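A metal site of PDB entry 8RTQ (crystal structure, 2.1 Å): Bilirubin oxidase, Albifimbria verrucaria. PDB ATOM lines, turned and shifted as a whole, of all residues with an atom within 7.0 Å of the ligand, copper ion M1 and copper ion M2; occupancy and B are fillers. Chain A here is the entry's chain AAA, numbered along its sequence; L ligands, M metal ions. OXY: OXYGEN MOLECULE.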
ATOM      1  N   HIS A  94      20.579   4.063   6.195  1.00  0.00           N
ATOM      2  CA  HIS A  94      20.050   4.088   7.586  1.00  0.00           C
ATOM      3  C   HIS A  94      20.903   5.037   8.436  1.00  0.00           C
ATOM      4  O   HIS A  94      22.136   4.875   8.449  1.00  0.00           O
ATOM      5  CB  HIS A  94      20.096   2.693   8.174  1.00  0.00           C
ATOM      6  CG  HIS A  94      19.825   2.694   9.631  1.00  0.00           C
ATOM      7  ND1 HIS A  94      18.628   3.153  10.147  1.00  0.00           N
ATOM      8  CD2 HIS A  94      20.519   2.195  10.672  1.00  0.00           C
ATOM      9  CE1 HIS A  94      18.639   2.982  11.460  1.00  0.00           C
ATOM     10  NE2 HIS A  94      19.782   2.399  11.800  1.00  0.00           N
ATOM     11  N   LEU A  95      20.263   5.995   9.108  1.00  0.00           N
ATOM     12  CA  LEU A  95      20.891   6.806  10.187  1.00  0.00           C
ATOM     13  C   LEU A  95      20.716   6.032  11.484  1.00  0.00           C
ATOM     14  O   LEU A  95      19.656   6.099  12.112  1.00  0.00           O
ATOM     15  CB  LEU A  95      20.245   8.194  10.254  1.00  0.00           C
ATOM     16  CG  LEU A  95      20.890   9.175  11.235  1.00  0.00           C
ATOM     17  CD1 LEU A  95      22.365   9.304  10.937  1.00  0.00           C
ATOM     18  CD2 LEU A  95      20.240  10.553  11.151  1.00  0.00           C
ATOM     19  N   HIS A  96      21.717   5.251  11.822  1.00  0.00           N
ATOM     20  CA  HIS A  96      21.796   4.484  13.083  1.00  0.00           C
ATOM     21  C   HIS A  96      21.888   5.441  14.286  1.00  0.00           C
ATOM     22  O   HIS A  96      22.884   6.194  14.392  1.00  0.00           O
ATOM     23  CB  HIS A  96      22.948   3.473  12.965  1.00  0.00           C
ATOM     24  CG  HIS A  96      22.979   2.454  14.044  1.00  0.00           C
ATOM     25  ND1 HIS A  96      23.282   1.160  13.802  1.00  0.00           N
ATOM     26  CD2 HIS A  96      22.750   2.557  15.373  1.00  0.00           C
ATOM     27  CE1 HIS A  96      23.269   0.484  14.931  1.00  0.00           C
ATOM     28  NE2 HIS A  96      22.936   1.318  15.916  1.00  0.00           N
ATOM     29  N   GLY A  97      20.903   5.375  15.187  1.00  0.00           N
ATOM     30  CA  GLY A  97      20.820   6.186  16.406  1.00  0.00           C
ATOM     31  C   GLY A  97      19.757   7.265  16.313  1.00  0.00           C
ATOM     32  O   GLY A  97      19.601   8.009  17.287  1.00  0.00           O
ATOM     33  N   ASP A 105      14.157   5.409   7.388  1.00  0.00           N
ATOM     34  CA  ASP A 105      15.004   4.703   8.390  1.00  0.00           C
ATOM     35  C   ASP A 105      15.961   3.716   7.745  1.00  0.00           C
ATOM     36  O   ASP A 105      16.786   3.143   8.479  1.00  0.00           O
ATOM     37  CB  ASP A 105      14.128   3.991   9.430  1.00  0.00           C
ATOM     38  CG  ASP A 105      14.902   3.519  10.646  1.00  0.00           C
ATOM     39  OD1 ASP A 105      15.718   4.300  11.173  1.00  0.00           O
ATOM     40  OD2 ASP A 105      14.641   2.344  11.069  1.00  0.00           O
ATOM     41  N   GLY A 106      15.870   3.505   6.426  1.00  0.00           N
ATOM     42  CA  GLY A 106      16.690   2.538   5.675  1.00  0.00           C
ATOM     43  C   GLY A 106      16.169   1.101   5.786  1.00  0.00           C
ATOM     44  O   GLY A 106      16.984   0.162   5.781  1.00  0.00           O
ATOM     45  N   TRP A 132      25.671   7.261  13.224  1.00  0.00           N
ATOM     46  CA  TRP A 132      26.437   6.978  11.996  1.00  0.00           C
ATOM     47  C   TRP A 132      25.412   6.540  10.957  1.00  0.00           C
ATOM     48  O   TRP A 132      24.306   6.065  11.359  1.00  0.00           O
ATOM     49  CB  TRP A 132      27.574   5.989  12.290  1.00  0.00           C
ATOM     50  CG  TRP A 132      27.164   4.581  12.640  1.00  0.00           C
ATOM     51  CD1 TRP A 132      26.409   4.163  13.708  1.00  0.00           C
ATOM     52  CD2 TRP A 132      27.598   3.381  11.969  1.00  0.00           C
ATOM     53  NE1 TRP A 132      26.320   2.809  13.718  1.00  0.00           N
ATOM     54  CE2 TRP A 132      27.028   2.292  12.655  1.00  0.00           C
ATOM     55  CE3 TRP A 132      28.408   3.130  10.847  1.00  0.00           C
ATOM     56  CZ2 TRP A 132      27.262   0.978  12.273  1.00  0.00           C
ATOM     57  CZ3 TRP A 132      28.619   1.834  10.453  1.00  0.00           C
ATOM     58  CH2 TRP A 132      28.028   0.771  11.151  1.00  0.00           C
ATOM     59  N   HIS A 134      24.835   4.496   7.253  1.00  0.00           N
ATOM     60  CA  HIS A 134      25.460   3.388   6.490  1.00  0.00           C
ATOM     61  C   HIS A 134      24.409   2.648   5.683  1.00  0.00           C
ATOM     62  O   HIS A 134      23.135   2.804   5.929  1.00  0.00           O
ATOM     63  CB  HIS A 134      26.206   2.456   7.437  1.00  0.00           C
ATOM     64  CG  HIS A 134      25.336   1.775   8.421  1.00  0.00           C
ATOM     65  ND1 HIS A 134      24.593   0.671   8.087  1.00  0.00           N
ATOM     66  CD2 HIS A 134      25.120   2.002   9.724  1.00  0.00           C
ATOM     67  CE1 HIS A 134      23.944   0.232   9.145  1.00  0.00           C
ATOM     68  NE2 HIS A 134      24.246   1.029  10.173  1.00  0.00           N
ATOM     69  N   ASP A 135      24.921   1.822   4.782  1.00  0.00           N
ATOM     70  CA  ASP A 135      24.043   1.129   3.847  1.00  0.00           C
ATOM     71  C   ASP A 135      23.299   0.030   4.600  1.00  0.00           C
ATOM     72  O   ASP A 135      23.819  -0.450   5.622  1.00  0.00           O
ATOM     73  CB  ASP A 135      24.794   0.587   2.646  1.00  0.00           C
ATOM     74  CG  ASP A 135      23.777   0.114   1.629  1.00  0.00           C
ATOM     75  OD1 ASP A 135      23.044   1.006   1.154  1.00  0.00           O
ATOM     76  OD2 ASP A 135      23.651  -1.127   1.468  1.00  0.00           O
ATOM     77  N   HIS A 136      22.095  -0.263   4.134  1.00  0.00           N
ATOM     78  CA  HIS A 136      21.213  -1.292   4.737  1.00  0.00           C
ATOM     79  C   HIS A 136      20.463  -2.084   3.645  1.00  0.00           C
ATOM     80  O   HIS A 136      19.498  -2.796   4.002  1.00  0.00           O
ATOM     81  CB  HIS A 136      20.287  -0.545   5.693  1.00  0.00           C
ATOM     82  CG  HIS A 136      19.901  -1.310   6.918  1.00  0.00           C
ATOM     83  ND1 HIS A 136      19.381  -2.577   6.855  1.00  0.00           N
ATOM     84  CD2 HIS A 136      19.983  -0.972   8.235  1.00  0.00           C
ATOM     85  CE1 HIS A 136      19.156  -3.007   8.086  1.00  0.00           C
ATOM     86  NE2 HIS A 136      19.504  -2.042   8.952  1.00  0.00           N
ATOM     87  N   THR A 141      24.283  -5.579   2.418  1.00  0.00           N
ATOM     88  CA  THR A 141      24.660  -4.579   3.424  1.00  0.00           C
ATOM     89  C   THR A 141      26.148  -4.751   3.788  1.00  0.00           C
ATOM     90  O   THR A 141      26.881  -3.746   3.817  1.00  0.00           O
ATOM     91  CB  THR A 141      23.736  -4.645   4.627  1.00  0.00           C
ATOM     92  OG1 THR A 141      22.425  -4.247   4.233  1.00  0.00           O
ATOM     93  CG2 THR A 141      24.217  -3.762   5.759  1.00  0.00           C
ATOM     94  N   ALA A 274      28.664  -1.787  15.578  1.00  0.00           N
ATOM     95  CA  ALA A 274      27.654  -0.709  15.526  1.00  0.00           C
ATOM     96  C   ALA A 274      27.576   0.021  16.876  1.00  0.00           C
ATOM     97  O   ALA A 274      26.912   1.050  16.943  1.00  0.00           O
ATOM     98  CB  ALA A 274      26.305  -1.243  15.080  1.00  0.00           C
ATOM     99  N   ARG A 276      28.797   2.623  19.560  1.00  0.00           N
ATOM    100  CA  ARG A 276      29.571   3.878  19.777  1.00  0.00           C
ATOM    101  C   ARG A 276      29.849   4.023  21.282  1.00  0.00           C
ATOM    102  O   ARG A 276      28.902   3.901  22.102  1.00  0.00           O
ATOM    103  CB  ARG A 276      28.842   5.116  19.226  1.00  0.00           C
ATOM    104  CG  ARG A 276      28.701   5.118  17.722  1.00  0.00           C
ATOM    105  CD  ARG A 276      27.517   4.276  17.303  1.00  0.00           C
ATOM    106  NE  ARG A 276      26.259   4.939  17.651  1.00  0.00           N
ATOM    107  CZ  ARG A 276      25.114   4.292  17.869  1.00  0.00           C
ATOM    108  NH1 ARG A 276      24.030   4.985  18.209  1.00  0.00           N
ATOM    109  NH2 ARG A 276      25.052   2.965  17.782  1.00  0.00           N
ATOM    110  N   HIS A 401      20.752  -5.187  17.663  1.00  0.00           N
ATOM    111  CA  HIS A 401      20.341  -3.787  17.433  1.00  0.00           C
ATOM    112  C   HIS A 401      18.840  -3.777  17.191  1.00  0.00           C
ATOM    113  O   HIS A 401      18.344  -4.637  16.453  1.00  0.00           O
ATOM    114  CB  HIS A 401      21.090  -3.217  16.231  1.00  0.00           C
ATOM    115  CG  HIS A 401      20.669  -1.843  15.873  1.00  0.00           C
ATOM    116  ND1 HIS A 401      20.503  -0.843  16.819  1.00  0.00           N
ATOM    117  CD2 HIS A 401      20.378  -1.292  14.667  1.00  0.00           C
ATOM    118  CE1 HIS A 401      20.173   0.286  16.202  1.00  0.00           C
ATOM    119  NE2 HIS A 401      20.069   0.024  14.869  1.00  0.00           N
ATOM    120  N   ILE A 402      18.163  -2.815  17.811  1.00  0.00           N
ATOM    121  CA  ILE A 402      16.717  -2.542  17.636  1.00  0.00           C
ATOM    122  C   ILE A 402      16.608  -1.115  17.123  1.00  0.00           C
ATOM    123  O   ILE A 402      17.025  -0.186  17.833  1.00  0.00           O
ATOM    124  CB  ILE A 402      15.987  -2.728  18.971  1.00  0.00           C
ATOM    125  CG1 ILE A 402      16.291  -4.090  19.605  1.00  0.00           C
ATOM    126  CG2 ILE A 402      14.485  -2.498  18.777  1.00  0.00           C
ATOM    127  CD1 ILE A 402      15.794  -4.248  21.054  1.00  0.00           C
ATOM    128  N   HIS A 403      16.019  -0.954  15.946  1.00  0.00           N
ATOM    129  CA  HIS A 403      15.716   0.371  15.341  1.00  0.00           C
ATOM    130  C   HIS A 403      14.695   1.129  16.215  1.00  0.00           C
ATOM    131  O   HIS A 403      14.090   0.516  17.083  1.00  0.00           O
ATOM    132  CB  HIS A 403      15.203   0.192  13.895  1.00  0.00           C
ATOM    133  CG  HIS A 403      16.270  -0.193  12.940  1.00  0.00           C
ATOM    134  ND1 HIS A 403      16.549   0.554  11.840  1.00  0.00           N
ATOM    135  CD2 HIS A 403      17.122  -1.248  12.910  1.00  0.00           C
ATOM    136  CE1 HIS A 403      17.517  -0.017  11.144  1.00  0.00           C
ATOM    137  NE2 HIS A 403      17.901  -1.125  11.775  1.00  0.00           N
ATOM    138  N   VAL A 431      22.565  -0.919  20.568  1.00  0.00           N
ATOM    139  CA  VAL A 431      23.188  -2.232  20.272  1.00  0.00           C
ATOM    140  C   VAL A 431      23.652  -2.863  21.588  1.00  0.00           C
ATOM    141  O   VAL A 431      24.133  -2.152  22.449  1.00  0.00           O
ATOM    142  CB  VAL A 431      24.373  -2.052  19.313  1.00  0.00           C
ATOM    143  CG1 VAL A 431      25.029  -3.380  18.936  1.00  0.00           C
ATOM    144  CG2 VAL A 431      23.939  -1.291  18.070  1.00  0.00           C
ATOM    145  N   MET A 454      13.057  -2.611  11.866  1.00  0.00           N
ATOM    146  CA  MET A 454      13.930  -3.798  11.838  1.00  0.00           C
ATOM    147  C   MET A 454      14.598  -3.932  13.190  1.00  0.00           C
ATOM    148  O   MET A 454      14.648  -2.968  13.942  1.00  0.00           O
ATOM    149  CB  MET A 454      14.984  -3.639  10.738  1.00  0.00           C
ATOM    150  CG  MET A 454      14.352  -3.550   9.339  1.00  0.00           C
ATOM    151  SD  MET A 454      15.598  -3.352   8.046  1.00  0.00           S
ATOM    152  CE  MET A 454      16.247  -1.748   8.480  1.00  0.00           C
ATOM    153  N   PHE A 455      14.951  -5.158  13.551  1.00  0.00           N
ATOM    154  CA  PHE A 455      15.919  -5.492  14.618  1.00  0.00           C
ATOM    155  C   PHE A 455      16.660  -6.726  14.101  1.00  0.00           C
ATOM    156  O   PHE A 455      16.117  -7.476  13.267  1.00  0.00           O
ATOM    157  CB  PHE A 455      15.260  -5.712  15.976  1.00  0.00           C
ATOM    158  CG  PHE A 455      14.402  -6.946  16.123  1.00  0.00           C
ATOM    159  CD1 PHE A 455      13.126  -7.003  15.571  1.00  0.00           C
ATOM    160  CD2 PHE A 455      14.853  -8.040  16.836  1.00  0.00           C
ATOM    161  CE1 PHE A 455      12.330  -8.122  15.727  1.00  0.00           C
ATOM    162  CE2 PHE A 455      14.044  -9.154  17.027  1.00  0.00           C
ATOM    163  CZ  PHE A 455      12.774  -9.196  16.470  1.00  0.00           C
ATOM    164  N   HIS A 456      17.914  -6.853  14.491  1.00  0.00           N
ATOM    165  CA  HIS A 456      18.821  -7.812  13.869  1.00  0.00           C
ATOM    166  C   HIS A 456      20.134  -7.812  14.605  1.00  0.00           C
ATOM    167  O   HIS A 456      20.409  -6.876  15.411  1.00  0.00           O
ATOM    168  CB  HIS A 456      19.043  -7.448  12.405  1.00  0.00           C
ATOM    169  CG  HIS A 456      19.583  -6.077  12.200  1.00  0.00           C
ATOM    170  ND1 HIS A 456      20.914  -5.815  12.077  1.00  0.00           N
ATOM    171  CD2 HIS A 456      18.947  -4.890  12.093  1.00  0.00           C
ATOM    172  CE1 HIS A 456      21.087  -4.536  11.853  1.00  0.00           C
ATOM    173  NE2 HIS A 456      19.886  -3.942  11.876  1.00  0.00           N
ATOM    174  N   CYS A 457      20.900  -8.834  14.297  1.00  0.00           N
ATOM    175  CA  CYS A 457      22.346  -8.867  14.560  1.00  0.00           C
ATOM    176  C   CYS A 457      23.025  -7.850  13.624  1.00  0.00           C
ATOM    177  O   CYS A 457      22.612  -7.765  12.437  1.00  0.00           O
ATOM    178  CB  CYS A 457      22.854 -10.294  14.426  1.00  0.00           C
ATOM    179  SG  CYS A 457      24.627 -10.347  14.717  1.00  0.00           S
ATOM    180  N   HIS A 458      24.049  -7.139  14.100  1.00  0.00           N
ATOM    181  CA  HIS A 458      24.843  -6.160  13.321  1.00  0.00           C
ATOM    182  C   HIS A 458      26.210  -6.743  12.954  1.00  0.00           C
ATOM    183  O   HIS A 458      27.047  -5.971  12.389  1.00  0.00           O
ATOM    184  CB  HIS A 458      24.940  -4.819  14.068  1.00  0.00           C
ATOM    185  CG  HIS A 458      24.968  -3.619  13.186  1.00  0.00           C
ATOM    186  ND1 HIS A 458      26.027  -3.353  12.349  1.00  0.00           N
ATOM    187  CD2 HIS A 458      24.101  -2.584  13.066  1.00  0.00           C
ATOM    188  CE1 HIS A 458      25.780  -2.226  11.709  1.00  0.00           C
ATOM    189  NE2 HIS A 458      24.614  -1.732  12.134  1.00  0.00           N
ATOM    190  N   LEU A 460      27.434  -8.098   9.928  1.00  0.00           N
ATOM    191  CA  LEU A 460      26.732  -7.786   8.673  1.00  0.00           C
ATOM    192  C   LEU A 460      26.609  -9.079   7.847  1.00  0.00           C
ATOM    193  O   LEU A 460      25.643  -9.166   7.044  1.00  0.00           O
ATOM    194  CB  LEU A 460      27.443  -6.655   7.915  1.00  0.00           C
ATOM    195  CG  LEU A 460      27.534  -5.329   8.667  1.00  0.00           C
ATOM    196  CD1 LEU A 460      28.256  -4.301   7.830  1.00  0.00           C
ATOM    197  CD2 LEU A 460      26.155  -4.812   9.037  1.00  0.00           C
ATOM    198  N   GLU A 463      23.556 -10.662   9.330  1.00  0.00           N
ATOM    199  CA  GLU A 463      22.405  -9.801   8.952  1.00  0.00           C
ATOM    200  C   GLU A 463      21.977 -10.125   7.509  1.00  0.00           C
ATOM    201  O   GLU A 463      20.795 -10.251   7.291  1.00  0.00           O
ATOM    202  CB  GLU A 463      22.828  -8.341   9.078  1.00  0.00           C
ATOM    203  CG  GLU A 463      21.676  -7.366   8.957  1.00  0.00           C
ATOM    204  CD  GLU A 463      22.132  -5.919   8.950  1.00  0.00           C
ATOM    205  OE1 GLU A 463      22.990  -5.556   9.817  1.00  0.00           O
ATOM    206  OE2 GLU A 463      21.601  -5.153   8.081  1.00  0.00           O
ATOM    207  N   MET A 468      17.647 -11.139  10.788  1.00  0.00           N
ATOM    208  CA  MET A 468      16.937  -9.852  10.845  1.00  0.00           C
ATOM    209  C   MET A 468      15.434 -10.089  10.758  1.00  0.00           C
ATOM    210  O   MET A 468      15.010 -10.997  10.025  1.00  0.00           O
ATOM    211  CB  MET A 468      17.401  -8.972   9.688  1.00  0.00           C
ATOM    212  CG  MET A 468      16.842  -7.556   9.711  1.00  0.00           C
ATOM    213  SD  MET A 468      17.908  -6.511   8.649  1.00  0.00           S
ATOM    214  CE  MET A 468      17.372  -7.008   7.009  1.00  0.00           C
HETATM  215  O1  OXY L   1      21.737  -0.945  10.919  1.00  0.00           O
HETATM  216  O2  OXY L   1      21.331  -0.829  11.957  1.00  0.00           O
HETATM  217 CU    CU M   1      19.498  -2.007  10.981  1.00  0.00          CU
HETATM  218 CU    CU M   2      23.664   0.256  12.018  1.00  0.00          CU
HETATM  219 CU    CU M   3      19.984   1.149  13.290  1.00  0.00          CU
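Copper ion M2 is bound by ND1 of His 96 (2.0 Å), NE2 of His 134 (2.1 Å), NE2 of His 458 (2.2 Å) and O1 of the ligand (2.5 Å).
His 94 touches copper ion M2 (CD2 to CU, 3.9 Å).
CZ2 of Trp 132 touches copper ion M2 (3.7 Å).
Within 4 Å of copper ion M2: His 94, His 96, Trp 132, His 134 and His 458.
The nearest printed residue that does not touch copper ion M2 is Ala 274 (4.3 Å).
A ring nitrogen (NE2) of His 401 sits close to an oxygen (O2) of the ligand, at 3.3 Å.
His 94 touches the ligand (CD2 to O1, 3.4 Å).
Hydrophobic or aromatic side chains that line the ligand: His 94, His 96, His 134, His 136, His 401, His 403, His 456 and His 458.
Of the 25 residues printed, 8 come within 4 Å of the ligand.
O of His 456 is in hydrogen-bond range of N of His 401 (2.8 Å).
ND1 of His 456 sits close to OE1 of Glu 463, at 3.1 Å.
A ring nitrogen (NE2) of His 96 sits at hydrogen-bond distance from the guanidinium group (NH2) of Arg 276.
The backbone carbonyl oxygen of Met 454 sits at hydrogen-bond distance from the backbone NH of His 403 (3.2 Å).
ND1 of His 401 lies close to NE2 of His 96.
The backbone NH of His 94 is in hydrogen-bond range of the backbone carbonyl oxygen of His 134.
A ring nitrogen (ND1) of His 94 lies within hydrogen-bond range of the backbone carbonyl oxygen (O) of Asp 105 (2.5 Å).
N of His 96 sits close to NE2 of His 94 (3.4 Å).
Merely in contact with copper ion M1: His 401 (3.9 Å).
Within 4 Å of copper ion M1: His 136, His 401, His 403 and His 456.
NE2 of His 403 is bound to copper ion M1 (2.0 Å).
NE2 of His 136 is bound to copper ion M1 (2.0 Å).
Copper ion M1 is bound by a ring nitrogen (NE2) of His 456, at 2.2 Å.
An oxygen (O2) of the ligand binds copper ion M1 (2.4 Å).
Copper ion M1 has four donor atoms within binding distance.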
